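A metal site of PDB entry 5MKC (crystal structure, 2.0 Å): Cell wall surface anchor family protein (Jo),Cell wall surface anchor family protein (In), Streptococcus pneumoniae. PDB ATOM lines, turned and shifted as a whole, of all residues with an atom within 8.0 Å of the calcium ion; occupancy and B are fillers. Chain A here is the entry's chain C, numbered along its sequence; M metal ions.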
ATOM      1  N   GLN A 119     -18.088   3.529  11.885  1.00  0.00           N
ATOM      2  CA  GLN A 119     -19.458   3.465  12.420  1.00  0.00           C
ATOM      3  C   GLN A 119     -20.157   4.816  12.238  1.00  0.00           C
ATOM      4  O   GLN A 119     -19.650   5.848  12.703  1.00  0.00           O
ATOM      5  CB  GLN A 119     -19.463   3.057  13.873  1.00  0.00           C
ATOM      6  CG  GLN A 119     -18.764   1.718  14.105  1.00  0.00           C
ATOM      7  CD  GLN A 119     -19.301   0.548  13.251  1.00  0.00           C
ATOM      8  OE1 GLN A 119     -18.944   0.373  12.071  1.00  0.00           O
ATOM      9  NE2 GLN A 119     -20.112  -0.268  13.866  1.00  0.00           N
ATOM     10  N   LEU A 120     -21.294   4.817  11.571  1.00  0.00           N
ATOM     11  CA  LEU A 120     -21.953   6.050  11.128  1.00  0.00           C
ATOM     12  C   LEU A 120     -23.388   6.198  11.699  1.00  0.00           C
ATOM     13  O   LEU A 120     -24.081   7.174  11.426  1.00  0.00           O
ATOM     14  CB  LEU A 120     -22.065   6.064   9.586  1.00  0.00           C
ATOM     15  CG  LEU A 120     -20.743   5.899   8.837  1.00  0.00           C
ATOM     16  CD1 LEU A 120     -20.957   5.735   7.356  1.00  0.00           C
ATOM     17  CD2 LEU A 120     -19.780   7.048   9.093  1.00  0.00           C
ATOM     18  N   GLY A 121     -23.873   5.203  12.405  1.00  0.00           N
ATOM     19  CA  GLY A 121     -25.322   5.142  12.714  1.00  0.00           C
ATOM     20  C   GLY A 121     -26.337   5.395  11.566  1.00  0.00           C
ATOM     21  O   GLY A 121     -26.069   5.165  10.386  1.00  0.00           O
ATOM     22  N   THR A 122     -27.492   5.920  11.951  1.00  0.00           N
ATOM     23  CA  THR A 122     -28.737   5.713  11.227  1.00  0.00           C
ATOM     24  C   THR A 122     -28.704   6.296   9.833  1.00  0.00           C
ATOM     25  O   THR A 122     -29.183   5.676   8.878  1.00  0.00           O
ATOM     26  CB  THR A 122     -29.910   6.414  11.974  1.00  0.00           C
ATOM     27  OG1 THR A 122     -30.055   5.827  13.254  1.00  0.00           O
ATOM     28  CG2 THR A 122     -31.233   6.285  11.239  1.00  0.00           C
ATOM     29  N   ASP A 123     -28.225   7.525   9.712  1.00  0.00           N
ATOM     30  CA  ASP A 123     -28.333   8.232   8.438  1.00  0.00           C
ATOM     31  C   ASP A 123     -27.206   7.879   7.456  1.00  0.00           C
ATOM     32  O   ASP A 123     -27.200   8.387   6.331  1.00  0.00           O
ATOM     33  CB  ASP A 123     -28.407   9.742   8.670  1.00  0.00           C
ATOM     34  CG  ASP A 123     -27.147  10.308   9.292  1.00  0.00           C
ATOM     35  OD1 ASP A 123     -26.319   9.493   9.705  1.00  0.00           O
ATOM     36  OD2 ASP A 123     -27.019  11.546   9.357  1.00  0.00           O
ATOM     37  N   GLY A 124     -26.261   7.037   7.871  1.00  0.00           N
ATOM     38  CA  GLY A 124     -25.142   6.645   7.008  1.00  0.00           C
ATOM     39  C   GLY A 124     -24.150   7.759   6.676  1.00  0.00           C
ATOM     40  O   GLY A 124     -23.424   7.674   5.678  1.00  0.00           O
ATOM     41  N   ARG A 125     -24.123   8.795   7.504  1.00  0.00           N
ATOM     42  CA  ARG A 125     -23.135   9.871   7.385  1.00  0.00           C
ATOM     43  C   ARG A 125     -22.350  10.026   8.676  1.00  0.00           C
ATOM     44  O   ARG A 125     -22.787   9.598   9.743  1.00  0.00           O
ATOM     45  CB  ARG A 125     -23.824  11.196   7.036  1.00  0.00           C
ATOM     46  CG  ARG A 125     -24.444  11.129   5.628  1.00  0.00           C
ATOM     47  CD  ARG A 125     -24.975  12.480   5.202  1.00  0.00           C
ATOM     48  NE  ARG A 125     -26.148  12.811   5.985  1.00  0.00           N
ATOM     49  CZ  ARG A 125     -27.402  12.528   5.628  1.00  0.00           C
ATOM     50  NH1 ARG A 125     -27.677  11.927   4.464  1.00  0.00           N
ATOM     51  NH2 ARG A 125     -28.399  12.885   6.433  1.00  0.00           N
ATOM     52  N   PHE A 126     -21.163  10.616   8.590  1.00  0.00           N
ATOM     53  CA  PHE A 126     -20.306  10.774   9.783  1.00  0.00           C
ATOM     54  C   PHE A 126     -20.665  12.100  10.426  1.00  0.00           C
ATOM     55  O   PHE A 126     -20.276  13.162   9.950  1.00  0.00           O
ATOM     56  CB  PHE A 126     -18.837  10.789   9.360  1.00  0.00           C
ATOM     57  CG  PHE A 126     -17.833  10.649  10.469  1.00  0.00           C
ATOM     58  CD1 PHE A 126     -17.892   9.608  11.383  1.00  0.00           C
ATOM     59  CD2 PHE A 126     -16.706  11.453  10.492  1.00  0.00           C
ATOM     60  CE1 PHE A 126     -16.894   9.427  12.324  1.00  0.00           C
ATOM     61  CE2 PHE A 126     -15.718  11.291  11.425  1.00  0.00           C
ATOM     62  CZ  PHE A 126     -15.807  10.275  12.348  1.00  0.00           C
ATOM     63  N   ASP A 127     -21.443  12.037  11.505  1.00  0.00           N
ATOM     64  CA  ASP A 127     -21.996  13.210  12.158  1.00  0.00           C
ATOM     65  C   ASP A 127     -21.350  13.397  13.533  1.00  0.00           C
ATOM     66  O   ASP A 127     -20.659  12.522  13.994  1.00  0.00           O
ATOM     67  CB  ASP A 127     -23.496  12.995  12.351  1.00  0.00           C
ATOM     68  CG  ASP A 127     -24.233  12.815  11.047  1.00  0.00           C
ATOM     69  OD1 ASP A 127     -23.954  13.545  10.073  1.00  0.00           O
ATOM     70  OD2 ASP A 127     -25.150  11.976  11.014  1.00  0.00           O
ATOM     71  N   PRO A 128     -21.593  14.544  14.196  1.00  0.00           N
ATOM     72  CA  PRO A 128     -21.037  14.772  15.517  1.00  0.00           C
ATOM     73  C   PRO A 128     -21.249  13.653  16.522  1.00  0.00           C
ATOM     74  O   PRO A 128     -20.370  13.392  17.349  1.00  0.00           O
ATOM     75  CB  PRO A 128     -21.724  16.059  15.945  1.00  0.00           C
ATOM     76  CG  PRO A 128     -21.769  16.826  14.640  1.00  0.00           C
ATOM     77  CD  PRO A 128     -22.172  15.786  13.638  1.00  0.00           C
ATOM     78  N   ALA A 129     -22.388  12.990  16.448  1.00  0.00           N
ATOM     79  CA  ALA A 129     -22.668  11.852  17.339  1.00  0.00           C
ATOM     80  C   ALA A 129     -21.711  10.673  17.141  1.00  0.00           C
ATOM     81  O   ALA A 129     -21.634   9.814  17.985  1.00  0.00           O
ATOM     82  CB  ALA A 129     -24.116  11.384  17.153  1.00  0.00           C
ATOM     83  N   ASP A 130     -20.970  10.633  16.029  1.00  0.00           N
ATOM     84  CA  ASP A 130     -20.157   9.461  15.685  1.00  0.00           C
ATOM     85  C   ASP A 130     -18.656   9.620  15.986  1.00  0.00           C
ATOM     86  O   ASP A 130     -17.861   8.716  15.673  1.00  0.00           O
ATOM     87  CB  ASP A 130     -20.351   9.110  14.217  1.00  0.00           C
ATOM     88  CG  ASP A 130     -21.822   9.023  13.830  1.00  0.00           C
ATOM     89  OD1 ASP A 130     -22.632   8.355  14.493  1.00  0.00           O
ATOM     90  OD2 ASP A 130     -22.225   9.664  12.861  1.00  0.00           O
ATOM     91  N   TYR A 131     -18.269  10.755  16.548  1.00  0.00           N
ATOM     92  CA  TYR A 131     -16.853  11.054  16.815  1.00  0.00           C
ATOM     93  C   TYR A 131     -16.736  12.026  18.008  1.00  0.00           C
ATOM     94  O   TYR A 131     -17.706  12.641  18.388  1.00  0.00           O
ATOM     95  CB  TYR A 131     -16.156  11.635  15.590  1.00  0.00           C
ATOM     96  CG  TYR A 131     -16.576  13.059  15.238  1.00  0.00           C
ATOM     97  CD1 TYR A 131     -17.410  13.316  14.151  1.00  0.00           C
ATOM     98  CD2 TYR A 131     -16.082  14.167  15.935  1.00  0.00           C
ATOM     99  CE1 TYR A 131     -17.764  14.611  13.785  1.00  0.00           C
ATOM    100  CE2 TYR A 131     -16.443  15.468  15.591  1.00  0.00           C
ATOM    101  CZ  TYR A 131     -17.296  15.679  14.524  1.00  0.00           C
ATOM    102  OH  TYR A 131     -17.712  16.956  14.241  1.00  0.00           O
HETATM  103 CA    CA M   1     -24.487   9.562  11.719  1.00  0.00          CA
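Within 4 Å of the calcium ion: Leu 120, Asp 123, Arg 125, Asp 127 and Asp 130.
The calcium ion is bound by O of Leu 120 (2.4 Å), OD2 of Asp 130 (2.5 Å), OD2 of Asp 127 (2.6 Å), O of Arg 125 (2.6 Å) and OD1 of Asp 123 (2.7 Å).
The calcium ion has five donor atoms within binding distance.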
